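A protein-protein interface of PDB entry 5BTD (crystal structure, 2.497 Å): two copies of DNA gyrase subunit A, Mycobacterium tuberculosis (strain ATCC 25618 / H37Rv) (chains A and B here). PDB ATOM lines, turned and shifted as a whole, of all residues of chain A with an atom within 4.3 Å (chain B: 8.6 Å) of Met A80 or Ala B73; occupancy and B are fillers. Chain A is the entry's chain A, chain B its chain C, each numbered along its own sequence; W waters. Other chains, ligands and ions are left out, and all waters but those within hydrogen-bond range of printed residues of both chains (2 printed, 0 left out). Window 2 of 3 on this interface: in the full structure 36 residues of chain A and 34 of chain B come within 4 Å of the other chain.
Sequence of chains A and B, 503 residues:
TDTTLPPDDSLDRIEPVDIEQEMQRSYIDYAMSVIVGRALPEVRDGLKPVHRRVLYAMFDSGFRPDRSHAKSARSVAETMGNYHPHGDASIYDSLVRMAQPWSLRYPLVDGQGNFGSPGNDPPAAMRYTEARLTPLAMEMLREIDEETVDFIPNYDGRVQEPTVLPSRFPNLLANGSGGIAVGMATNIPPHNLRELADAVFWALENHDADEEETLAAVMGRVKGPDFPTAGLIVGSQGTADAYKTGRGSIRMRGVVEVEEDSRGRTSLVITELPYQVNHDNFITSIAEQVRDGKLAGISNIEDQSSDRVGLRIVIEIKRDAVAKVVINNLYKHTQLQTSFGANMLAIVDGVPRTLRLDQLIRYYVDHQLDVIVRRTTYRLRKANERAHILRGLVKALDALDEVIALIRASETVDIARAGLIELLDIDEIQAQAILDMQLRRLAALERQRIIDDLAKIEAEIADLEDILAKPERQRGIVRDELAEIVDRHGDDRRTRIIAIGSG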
ATOM      1  N   VAL A  76       6.174   5.174  28.867  1.00  0.00           N
ATOM      2  CA  VAL A  76       6.994   5.229  27.661  1.00  0.00           C
ATOM      3  C   VAL A  76       7.570   3.857  27.343  1.00  0.00           C
ATOM      4  O   VAL A  76       7.454   3.373  26.219  1.00  0.00           O
ATOM      5  CB  VAL A  76       8.150   6.238  27.796  1.00  0.00           C
ATOM      6  CG1 VAL A  76       9.064   6.172  26.574  1.00  0.00           C
ATOM      7  CG2 VAL A  76       7.613   7.642  27.972  1.00  0.00           C
ATOM      8  N   ALA A  77       8.179   3.231  28.343  1.00  0.00           N
ATOM      9  CA  ALA A  77       8.838   1.946  28.149  1.00  0.00           C
ATOM     10  C   ALA A  77       7.831   0.889  27.712  1.00  0.00           C
ATOM     11  O   ALA A  77       8.130   0.065  26.850  1.00  0.00           O
ATOM     12  CB  ALA A  77       9.558   1.513  29.429  1.00  0.00           C
ATOM     13  N   GLU A  78       6.633   0.921  28.292  1.00  0.00           N
ATOM     14  CA  GLU A  78       5.596  -0.046  27.938  1.00  0.00           C
ATOM     15  C   GLU A  78       5.111   0.175  26.513  1.00  0.00           C
ATOM     16  O   GLU A  78       4.827  -0.782  25.790  1.00  0.00           O
ATOM     17  CB  GLU A  78       4.411   0.034  28.904  1.00  0.00           C
ATOM     18  CG  GLU A  78       4.465  -0.984  30.028  1.00  0.00           C
ATOM     19  CD  GLU A  78       4.266  -2.407  29.533  1.00  0.00           C
ATOM     20  OE1 GLU A  78       3.209  -2.690  28.923  1.00  0.00           O
ATOM     21  OE2 GLU A  78       5.173  -3.239  29.749  1.00  0.00           O
ATOM     22  N   THR A  79       5.003   1.438  26.115  1.00  0.00           N
ATOM     23  CA  THR A  79       4.586   1.766  24.762  1.00  0.00           C
ATOM     24  C   THR A  79       5.660   1.324  23.774  1.00  0.00           C
ATOM     25  O   THR A  79       5.377   0.681  22.760  1.00  0.00           O
ATOM     26  CB  THR A  79       4.331   3.276  24.604  1.00  0.00           C
ATOM     27  OG1 THR A  79       3.422   3.717  25.618  1.00  0.00           O
ATOM     28  CG2 THR A  79       3.750   3.588  23.233  1.00  0.00           C
ATOM     29  N   MET A  80       6.898   1.659  24.109  1.00  0.00           N
ATOM     30  CA  MET A  80       8.056   1.361  23.281  1.00  0.00           C
ATOM     31  C   MET A  80       8.279  -0.136  23.118  1.00  0.00           C
ATOM     32  O   MET A  80       8.582  -0.613  22.024  1.00  0.00           O
ATOM     33  CB  MET A  80       9.292   1.998  23.903  1.00  0.00           C
ATOM     34  CG  MET A  80      10.422   2.282  22.938  1.00  0.00           C
ATOM     35  SD  MET A  80      11.947   2.805  23.767  1.00  0.00           S
ATOM     36  CE  MET A  80      11.330   3.316  25.368  1.00  0.00           C
ATOM     37  N   GLY A  81       8.147  -0.866  24.220  1.00  0.00           N
ATOM     38  CA  GLY A  81       8.491  -2.274  24.263  1.00  0.00           C
ATOM     39  C   GLY A  81       7.491  -3.208  23.611  1.00  0.00           C
ATOM     40  O   GLY A  81       7.851  -4.319  23.223  1.00  0.00           O
ATOM     41  N   ASN A  82       6.240  -2.770  23.485  1.00  0.00           N
ATOM     42  CA  ASN A  82       5.173  -3.651  23.013  1.00  0.00           C
ATOM     43  C   ASN A  82       4.470  -3.208  21.729  1.00  0.00           C
ATOM     44  O   ASN A  82       4.015  -4.055  20.959  1.00  0.00           O
ATOM     45  CB  ASN A  82       4.120  -3.813  24.113  1.00  0.00           C
ATOM     46  CG  ASN A  82       4.603  -4.686  25.254  1.00  0.00           C
ATOM     47  OD1 ASN A  82       5.129  -4.189  26.252  1.00  0.00           O
ATOM     48  ND2 ASN A  82       4.441  -5.997  25.106  1.00  0.00           N
ATOM     49  N   HIS A  84       5.048   0.467  19.996  1.00  0.00           N
ATOM     50  CA  HIS A  84       5.625   1.544  19.197  1.00  0.00           C
ATOM     51  C   HIS A  84       7.143   1.386  19.030  1.00  0.00           C
ATOM     52  O   HIS A  84       7.913   1.804  19.894  1.00  0.00           O
ATOM     53  CB  HIS A  84       5.293   2.890  19.843  1.00  0.00           C
ATOM     54  CG  HIS A  84       5.270   4.029  18.875  1.00  0.00           C
ATOM     55  ND1 HIS A  84       4.529   3.998  17.714  1.00  0.00           N
ATOM     56  CD2 HIS A  84       5.894   5.232  18.892  1.00  0.00           C
ATOM     57  CE1 HIS A  84       4.697   5.131  17.056  1.00  0.00           C
ATOM     58  NE2 HIS A  84       5.521   5.897  17.750  1.00  0.00           N
ATOM     59  N   HIS A  86       9.881   2.704  18.287  1.00  0.00           N
ATOM     60  CA  HIS A  86      10.621   3.938  18.046  1.00  0.00           C
ATOM     61  C   HIS A  86      11.304   4.432  19.318  1.00  0.00           C
ATOM     62  O   HIS A  86      11.367   3.712  20.315  1.00  0.00           O
ATOM     63  CB  HIS A  86       9.681   5.005  17.486  1.00  0.00           C
ATOM     64  CG  HIS A  86       8.972   4.576  16.240  1.00  0.00           C
ATOM     65  ND1 HIS A  86       9.535   4.688  14.989  1.00  0.00           N
ATOM     66  CD2 HIS A  86       7.756   4.008  16.057  1.00  0.00           C
ATOM     67  CE1 HIS A  86       8.691   4.223  14.086  1.00  0.00           C
ATOM     68  NE2 HIS A  86       7.606   3.801  14.707  1.00  0.00           N
ATOM     69  N   ASP A  88      12.464   6.536  22.733  1.00  0.00           N
ATOM     70  CA  ASP A  88      11.824   6.916  23.991  1.00  0.00           C
ATOM     71  C   ASP A  88      11.584   8.421  24.088  1.00  0.00           C
ATOM     72  O   ASP A  88      10.594   8.859  24.674  1.00  0.00           O
ATOM     73  CB  ASP A  88      12.671   6.441  25.180  1.00  0.00           C
ATOM     74  CG  ASP A  88      14.117   6.892  25.095  1.00  0.00           C
ATOM     75  OD1 ASP A  88      14.847   6.355  24.232  1.00  0.00           O
ATOM     76  OD2 ASP A  88      14.530   7.759  25.900  1.00  0.00           O
ATOM     77  N   ILE A  91       8.466   9.691  22.001  1.00  0.00           N
ATOM     78  CA  ILE A  91       7.268   9.094  22.580  1.00  0.00           C
ATOM     79  C   ILE A  91       6.872   9.853  23.843  1.00  0.00           C
ATOM     80  O   ILE A  91       5.695  10.139  24.064  1.00  0.00           O
ATOM     81  CB  ILE A  91       7.475   7.599  22.901  1.00  0.00           C
ATOM     82  CG1 ILE A  91       7.551   6.798  21.603  1.00  0.00           C
ATOM     83  CG2 ILE A  91       6.344   7.066  23.791  1.00  0.00           C
ATOM     84  CD1 ILE A  91       7.949   5.357  21.787  1.00  0.00           C
ATOM     85  N   TYR A 155       4.214  -5.125  16.381  1.00  0.00           N
ATOM     86  CA  TYR A 155       5.278  -5.036  15.386  1.00  0.00           C
ATOM     87  C   TYR A 155       6.134  -6.300  15.299  1.00  0.00           C
ATOM     88  O   TYR A 155       6.887  -6.464  14.339  1.00  0.00           O
ATOM     89  CB  TYR A 155       6.164  -3.817  15.673  1.00  0.00           C
ATOM     90  CG  TYR A 155       6.900  -3.873  16.988  1.00  0.00           C
ATOM     91  CD1 TYR A 155       8.144  -4.487  17.093  1.00  0.00           C
ATOM     92  CD2 TYR A 155       6.356  -3.298  18.126  1.00  0.00           C
ATOM     93  CE1 TYR A 155       8.817  -4.536  18.302  1.00  0.00           C
ATOM     94  CE2 TYR A 155       7.017  -3.339  19.334  1.00  0.00           C
ATOM     95  CZ  TYR A 155       8.248  -3.958  19.419  1.00  0.00           C
ATOM     96  OH  TYR A 155       8.899  -3.993  20.628  1.00  0.00           O
ATOM     97  N   PHE B  63      11.800 -10.989  33.322  1.00  0.00           N
ATOM     98  CA  PHE B  63      12.808 -10.902  32.272  1.00  0.00           C
ATOM     99  C   PHE B  63      13.920 -11.910  32.543  1.00  0.00           C
ATOM    100  O   PHE B  63      15.058 -11.539  32.841  1.00  0.00           O
ATOM    101  CB  PHE B  63      13.376  -9.485  32.184  1.00  0.00           C
ATOM    102  CG  PHE B  63      12.332  -8.422  31.984  1.00  0.00           C
ATOM    103  CD1 PHE B  63      11.069  -8.740  31.498  1.00  0.00           C
ATOM    104  CD2 PHE B  63      12.615  -7.098  32.283  1.00  0.00           C
ATOM    105  CE1 PHE B  63      10.113  -7.759  31.319  1.00  0.00           C
ATOM    106  CE2 PHE B  63      11.665  -6.116  32.104  1.00  0.00           C
ATOM    107  CZ  PHE B  63      10.412  -6.446  31.619  1.00  0.00           C
ATOM    108  N   ALA B  70      13.547  -8.838  26.874  1.00  0.00           N
ATOM    109  CA  ALA B  70      12.653  -7.689  26.911  1.00  0.00           C
ATOM    110  C   ALA B  70      13.447  -6.446  26.529  1.00  0.00           C
ATOM    111  O   ALA B  70      14.663  -6.408  26.716  1.00  0.00           O
ATOM    112  CB  ALA B  70      12.035  -7.536  28.285  1.00  0.00           C
ATOM    113  N   LYS B  71      12.771  -5.437  25.982  1.00  0.00           N
ATOM    114  CA  LYS B  71      13.429  -4.170  25.677  1.00  0.00           C
ATOM    115  C   LYS B  71      14.049  -3.597  26.946  1.00  0.00           C
ATOM    116  O   LYS B  71      13.411  -3.558  27.995  1.00  0.00           O
ATOM    117  CB  LYS B  71      12.441  -3.176  25.064  1.00  0.00           C
ATOM    118  CG  LYS B  71      12.125  -3.454  23.602  1.00  0.00           C
ATOM    119  CD  LYS B  71      13.312  -3.136  22.698  1.00  0.00           C
ATOM    120  CE  LYS B  71      13.063  -3.584  21.263  1.00  0.00           C
ATOM    121  NZ  LYS B  71      14.265  -3.375  20.400  1.00  0.00           N
ATOM    122  N   SER B  72      15.302  -3.170  26.850  1.00  0.00           N
ATOM    123  CA  SER B  72      16.056  -2.784  28.036  1.00  0.00           C
ATOM    124  C   SER B  72      15.445  -1.555  28.707  1.00  0.00           C
ATOM    125  O   SER B  72      15.633  -1.338  29.905  1.00  0.00           O
ATOM    126  CB  SER B  72      17.522  -2.533  27.680  1.00  0.00           C
ATOM    127  OG  SER B  72      17.650  -1.485  26.742  1.00  0.00           O
ATOM    128  N   ALA B  73      14.708  -0.761  27.932  1.00  0.00           N
ATOM    129  CA  ALA B  73      13.990   0.394  28.468  1.00  0.00           C
ATOM    130  C   ALA B  73      13.007  -0.039  29.542  1.00  0.00           C
ATOM    131  O   ALA B  73      12.788   0.676  30.519  1.00  0.00           O
ATOM    132  CB  ALA B  73      13.257   1.138  27.359  1.00  0.00           C
ATOM    133  N   ARG B  74      12.407  -1.210  29.354  1.00  0.00           N
ATOM    134  CA  ARG B  74      11.443  -1.721  30.321  1.00  0.00           C
ATOM    135  C   ARG B  74      12.105  -2.079  31.650  1.00  0.00           C
ATOM    136  O   ARG B  74      11.507  -1.884  32.709  1.00  0.00           O
ATOM    137  CB  ARG B  74      10.713  -2.942  29.768  1.00  0.00           C
ATOM    138  CG  ARG B  74       9.850  -2.650  28.558  1.00  0.00           C
ATOM    139  CD  ARG B  74       9.200  -3.916  28.056  1.00  0.00           C
ATOM    140  NE  ARG B  74       8.327  -4.488  29.073  1.00  0.00           N
ATOM    141  CZ  ARG B  74       7.681  -5.643  28.949  1.00  0.00           C
ATOM    142  NH1 ARG B  74       7.808  -6.369  27.844  1.00  0.00           N
ATOM    143  NH2 ARG B  74       6.910  -6.074  29.938  1.00  0.00           N
ATOM    144  N   SER B  75      13.328  -2.604  31.594  1.00  0.00           N
ATOM    145  CA  SER B  75      14.070  -2.924  32.811  1.00  0.00           C
ATOM    146  C   SER B  75      14.441  -1.645  33.544  1.00  0.00           C
ATOM    147  O   SER B  75      14.305  -1.568  34.765  1.00  0.00           O
ATOM    148  CB  SER B  75      15.334  -3.737  32.500  1.00  0.00           C
ATOM    149  OG  SER B  75      15.007  -5.036  32.040  1.00  0.00           O
ATOM    150  N   VAL B  76      14.903  -0.647  32.796  1.00  0.00           N
ATOM    151  CA  VAL B  76      15.255   0.646  33.375  1.00  0.00           C
ATOM    152  C   VAL B  76      14.046   1.317  34.020  1.00  0.00           C
ATOM    153  O   VAL B  76      14.119   1.768  35.161  1.00  0.00           O
ATOM    154  CB  VAL B  76      15.849   1.593  32.318  1.00  0.00           C
ATOM    155  CG1 VAL B  76      16.076   2.985  32.900  1.00  0.00           C
ATOM    156  CG2 VAL B  76      17.151   1.027  31.772  1.00  0.00           C
ATOM    157  N   ALA B  77      12.944   1.393  33.280  1.00  0.00           N
ATOM    158  CA  ALA B  77      11.743   2.075  33.757  1.00  0.00           C
ATOM    159  C   ALA B  77      11.174   1.390  34.996  1.00  0.00           C
ATOM    160  O   ALA B  77      10.679   2.053  35.907  1.00  0.00           O
ATOM    161  CB  ALA B  77      10.688   2.144  32.650  1.00  0.00           C
ATOM    162  N   GLU B  78      11.225   0.061  35.017  1.00  0.00           N
ATOM    163  CA  GLU B  78      10.712  -0.698  36.151  1.00  0.00           C
ATOM    164  C   GLU B  78      11.585  -0.476  37.386  1.00  0.00           C
ATOM    165  O   GLU B  78      11.084  -0.411  38.507  1.00  0.00           O
ATOM    166  CB  GLU B  78      10.640  -2.191  35.819  1.00  0.00           C
ATOM    167  CG  GLU B  78       9.887  -3.016  36.861  1.00  0.00           C
ATOM    168  CD  GLU B  78       8.384  -2.773  36.841  1.00  0.00           C
ATOM    169  OE1 GLU B  78       7.891  -2.092  35.906  1.00  0.00           O
ATOM    170  OE2 GLU B  78       7.697  -3.268  37.767  1.00  0.00           O
ATOM    171  N   THR B  79      12.890  -0.372  37.175  1.00  0.00           N
ATOM    172  CA  THR B  79      13.819  -0.121  38.268  1.00  0.00           C
ATOM    173  C   THR B  79      13.560   1.270  38.838  1.00  0.00           C
ATOM    174  O   THR B  79      13.508   1.454  40.054  1.00  0.00           O
ATOM    175  CB  THR B  79      15.286  -0.238  37.808  1.00  0.00           C
ATOM    176  OG1 THR B  79      15.487  -1.495  37.154  1.00  0.00           O
ATOM    177  CG2 THR B  79      16.233  -0.134  38.996  1.00  0.00           C
ATOM    178  N   MET B  80      13.387   2.240  37.946  1.00  0.00           N
ATOM    179  CA  MET B  80      13.129   3.624  38.330  1.00  0.00           C
ATOM    180  C   MET B  80      11.830   3.780  39.099  1.00  0.00           C
ATOM    181  O   MET B  80      11.772   4.480  40.111  1.00  0.00           O
ATOM    182  CB  MET B  80      13.049   4.515  37.094  1.00  0.00           C
ATOM    183  CG  MET B  80      14.344   5.151  36.663  1.00  0.00           C
ATOM    184  SD  MET B  80      14.032   6.497  35.498  1.00  0.00           S
ATOM    185  CE  MET B  80      13.164   5.611  34.212  1.00  0.00           C
ATOM    186  N   ASP B  88      17.172   7.721  34.566  1.00  0.00           N
ATOM    187  CA  ASP B  88      17.155   6.570  33.667  1.00  0.00           C
ATOM    188  C   ASP B  88      18.503   6.361  32.981  1.00  0.00           C
ATOM    189  O   ASP B  88      18.906   5.225  32.730  1.00  0.00           O
ATOM    190  CB  ASP B  88      16.044   6.728  32.615  1.00  0.00           C
ATOM    191  CG  ASP B  88      16.106   8.051  31.880  1.00  0.00           C
ATOM    192  OD1 ASP B  88      15.783   9.088  32.497  1.00  0.00           O
ATOM    193  OD2 ASP B  88      16.451   8.053  30.679  1.00  0.00           O
ATOM    194  N   ILE B  91      21.147   4.657  35.280  1.00  0.00           N
ATOM    195  CA  ILE B  91      20.641   3.317  35.563  1.00  0.00           C
ATOM    196  C   ILE B  91      20.886   2.414  34.360  1.00  0.00           C
ATOM    197  O   ILE B  91      21.274   1.257  34.514  1.00  0.00           O
ATOM    198  CB  ILE B  91      19.138   3.321  35.914  1.00  0.00           C
ATOM    199  CG1 ILE B  91      18.933   3.913  37.303  1.00  0.00           C
ATOM    200  CG2 ILE B  91      18.560   1.897  35.877  1.00  0.00           C
ATOM    201  CD1 ILE B  91      17.488   4.144  37.668  1.00  0.00           C
ATOM    202  N   TYR B  92      20.650   2.940  33.164  1.00  0.00           N
ATOM    203  CA  TYR B  92      20.921   2.178  31.957  1.00  0.00           C
ATOM    204  C   TYR B  92      22.414   1.855  31.865  1.00  0.00           C
ATOM    205  O   TYR B  92      22.784   0.756  31.458  1.00  0.00           O
ATOM    206  CB  TYR B  92      20.457   2.935  30.708  1.00  0.00           C
ATOM    207  CG  TYR B  92      20.744   2.188  29.424  1.00  0.00           C
ATOM    208  CD1 TYR B  92      20.148   0.959  29.169  1.00  0.00           C
ATOM    209  CD2 TYR B  92      21.619   2.702  28.472  1.00  0.00           C
ATOM    210  CE1 TYR B  92      20.411   0.261  28.000  1.00  0.00           C
ATOM    211  CE2 TYR B  92      21.888   2.010  27.298  1.00  0.00           C
ATOM    212  CZ  TYR B  92      21.281   0.793  27.070  1.00  0.00           C
ATOM    213  OH  TYR B  92      21.542   0.104  25.911  1.00  0.00           O
ATOM    214  N   LEU B  95      23.124  -1.104  34.093  1.00  0.00           N
ATOM    215  CA  LEU B  95      22.597  -2.316  33.479  1.00  0.00           C
ATOM    216  C   LEU B  95      23.518  -2.778  32.356  1.00  0.00           C
ATOM    217  O   LEU B  95      23.832  -3.964  32.250  1.00  0.00           O
ATOM    218  CB  LEU B  95      21.182  -2.081  32.944  1.00  0.00           C
ATOM    219  CG  LEU B  95      20.541  -3.237  32.166  1.00  0.00           C
ATOM    220  CD1 LEU B  95      19.041  -3.261  32.407  1.00  0.00           C
ATOM    221  CD2 LEU B  95      20.816  -3.148  30.664  1.00  0.00           C
ATOM    222  N   ALA B 125      22.045   3.229  22.416  1.00  0.00           N
ATOM    223  CA  ALA B 125      21.070   3.828  23.308  1.00  0.00           C
ATOM    224  C   ALA B 125      20.041   2.802  23.749  1.00  0.00           C
ATOM    225  O   ALA B 125      19.855   1.765  23.111  1.00  0.00           O
ATOM    226  CB  ALA B 125      20.391   4.999  22.635  1.00  0.00           C
ATOM    227  N   MET B 126      19.372   3.129  24.844  1.00  0.00           N
ATOM    228  CA  MET B 126      18.355   2.291  25.462  1.00  0.00           C
ATOM    229  C   MET B 126      17.369   1.693  24.455  1.00  0.00           C
ATOM    230  O   MET B 126      17.019   0.516  24.537  1.00  0.00           O
ATOM    231  CB  MET B 126      17.600   3.138  26.490  1.00  0.00           C
ATOM    232  CG  MET B 126      16.717   2.378  27.445  1.00  0.00           C
ATOM    233  SD  MET B 126      16.067   3.473  28.728  1.00  0.00           S
ATOM    234  CE  MET B 126      15.093   4.617  27.756  1.00  0.00           C
ATOM    235  N   ARG B 127      16.943   2.508  23.498  1.00  0.00           N
ATOM    236  CA  ARG B 127      15.913   2.111  22.545  1.00  0.00           C
ATOM    237  C   ARG B 127      16.333   0.920  21.686  1.00  0.00           C
ATOM    238  O   ARG B 127      15.497   0.106  21.294  1.00  0.00           O
ATOM    239  CB  ARG B 127      15.555   3.296  21.646  1.00  0.00           C
ATOM    240  CG  ARG B 127      16.714   3.798  20.796  1.00  0.00           C
ATOM    241  CD  ARG B 127      16.372   5.098  20.074  1.00  0.00           C
ATOM    242  NE  ARG B 127      16.146   6.204  21.002  1.00  0.00           N
ATOM    243  CZ  ARG B 127      15.886   7.457  20.635  1.00  0.00           C
ATOM    244  NH1 ARG B 127      15.837   7.790  19.350  1.00  0.00           N
ATOM    245  NH2 ARG B 127      15.698   8.386  21.562  1.00  0.00           N
ATOM    246  N   PTR B 128      17.632   0.761  21.454  1.00  0.00           N
ATOM    247  CA  PTR B 128      18.104  -0.200  20.473  1.00  0.00           C
ATOM    248  C   PTR B 128      18.359  -1.539  21.086  1.00  0.00           C
ATOM    249  O   PTR B 128      18.368  -2.556  20.361  1.00  0.00           O
ATOM    250  CB  PTR B 128      19.430   0.240  19.871  1.00  0.00           C
ATOM    251  CG  PTR B 128      19.280   1.559  19.164  1.00  0.00           C
ATOM    252  CD1 PTR B 128      19.908   2.681  19.685  1.00  0.00           C
ATOM    253  CD2 PTR B 128      18.526   1.649  17.999  1.00  0.00           C
ATOM    254  CE1 PTR B 128      19.781   3.902  19.041  1.00  0.00           C
ATOM    255  CE2 PTR B 128      18.399   2.872  17.355  1.00  0.00           C
ATOM    256  CZ  PTR B 128      19.023   3.996  17.882  1.00  0.00           C
ATOM    257  OH  PTR B 128      18.916   5.204  17.255  1.00  0.00           O
ATOM    258  P   PTR B 128      20.274   5.862  16.698  1.00  0.00           P
ATOM    259  O1P PTR B 128      19.807   6.924  15.733  1.00  0.00           O
ATOM    260  O2P PTR B 128      20.950   6.391  17.940  1.00  0.00           O
ATOM    261  O3P PTR B 128      20.987   4.697  16.054  1.00  0.00           O
ATOM    262  N   THR B 129      18.581  -1.573  22.394  1.00  0.00           N
ATOM    263  CA  THR B 129      19.041  -2.799  23.038  1.00  0.00           C
ATOM    264  C   THR B 129      17.941  -3.533  23.793  1.00  0.00           C
ATOM    265  O   THR B 129      16.967  -2.934  24.246  1.00  0.00           O
ATOM    266  CB  THR B 129      20.191  -2.511  24.019  1.00  0.00           C
ATOM    267  OG1 THR B 129      19.697  -1.763  25.137  1.00  0.00           O
ATOM    268  CG2 THR B 129      21.299  -1.728  23.329  1.00  0.00           C
ATOM    269  N   GLU B 130      18.117  -4.844  23.918  1.00  0.00           N
ATOM    270  CA  GLU B 130      17.240  -5.680  24.725  1.00  0.00           C
ATOM    271  C   GLU B 130      18.079  -6.344  25.815  1.00  0.00           C
ATOM    272  O   GLU B 130      19.306  -6.361  25.736  1.00  0.00           O
ATOM    273  CB  GLU B 130      16.529  -6.731  23.865  1.00  0.00           C
ATOM    274  CG  GLU B 130      15.634  -6.147  22.794  1.00  0.00           C
ATOM    275  CD  GLU B 130      14.912  -7.213  22.000  1.00  0.00           C
ATOM    276  OE1 GLU B 130      15.337  -8.384  22.062  1.00  0.00           O
ATOM    277  OE2 GLU B 130      13.915  -6.883  21.318  1.00  0.00           O
ATOM    278  N   ALA B 131      17.425  -6.884  26.835  1.00  0.00           N
ATOM    279  CA  ALA B 131      18.151  -7.445  27.963  1.00  0.00           C
ATOM    280  C   ALA B 131      17.289  -8.359  28.814  1.00  0.00           C
ATOM    281  O   ALA B 131      16.070  -8.204  28.899  1.00  0.00           O
ATOM    282  CB  ALA B 131      18.721  -6.334  28.819  1.00  0.00           C
HETATM  283  O   HOH W   1       7.101  -3.761  31.653  1.00  0.00           O
HETATM  284  O   HOH W   2      17.218   5.252  23.655  1.00  0.00           O
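The side-chain carboxylate (OE2) of Glu A78 lies within salt-bridge range of the guanidinium group (NH2) of Arg B74 (3.3 Å). The guanidinium group of Arg B127 lies within salt-bridge range of the side-chain carboxylate of Asp A88.
O of Glu A78 sits close to OD1 of Asn A82 (3.5 Å). The backbone carbonyl oxygen (O) of Met B126 is in hydrogen-bond range of the side-chain hydroxyl (OG) of Ser B72. O of Gly A81 lies within hydrogen-bond range of OH of Tyr A155, at 2.8 Å. OE2 of Glu B130 lies within salt-bridge range of NZ of Lys B71 (3.6 Å).
Among the printed residues, pairs that only touch across the chains: Ala A77 with Ala B77 (3.5 Å), Ala A77 with Ala B73 (3.5 Å), Met A80 with Ala B73 (3.5 Å), Asp A88 with Met B126 (3.6 Å), Ala A77 with Arg B74 (3.6 Å), Asn A82 with Arg B74 (3.8 Å) and Gly A81 with Lys B71 (3.9 Å).
Of the printed residues of chain B, Glu A78 touches Arg B74. No residue of chain B comes within 4 Å of Thr A79. Met A80 touches just one residue of chain B: Ala B73 (3.5 Å). Of the printed residues of chain B, Asn A82 touches Arg B74 (3.8 Å). Ala B73 touches just these residues of chain A: Ala A77 (3.5 Å) and Met A80 (3.5 Å). Asp B88 touches none of the printed residues of chain A. The nearest printed residue of chain B that does not touch Met A80 is Arg B127 (4.2 Å).
Printed residues of chain A that touch a printed residue of chain B: Ala A77, Glu A78, Met A80, Gly A81, Asn A82 and Asp A88. Hydrophobic or aromatic side chains of chain A within 4 Å of the printed part of chain B: Ala A77 and Met A80. Of the 23 printed residues of chain B, 6 touch a printed residue of chain A. Hydrophobic or aromatic side chains of chain B that line the printed part of chain A: Ala B73, Ala B77 and Met B126. Along chain B the printed residues that touch a printed residue of chain A span positions 71 to 127. Among the printed residues, Asp or Glu carboxylates within 4 Å of a Lys or Arg side-chain nitrogen of the other chain: Glu A78 with Arg B74 (3.3 Å) and Asp A88 with Arg B127 (3.5 Å).
Ala B77 touches its own counterpart, Ala A77. 7 positions are printed for both chains.
Water W2 lies within hydrogen-bond range of the side-chain carboxylate (OD1) of Asp A88, the backbone NH (N) of Arg B127 and the backbone NH (N) of Met B126. Water W1 bridges OE2 of Glu A78 (2.8 Å) and NH2 of Arg B74 (2.9 Å).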
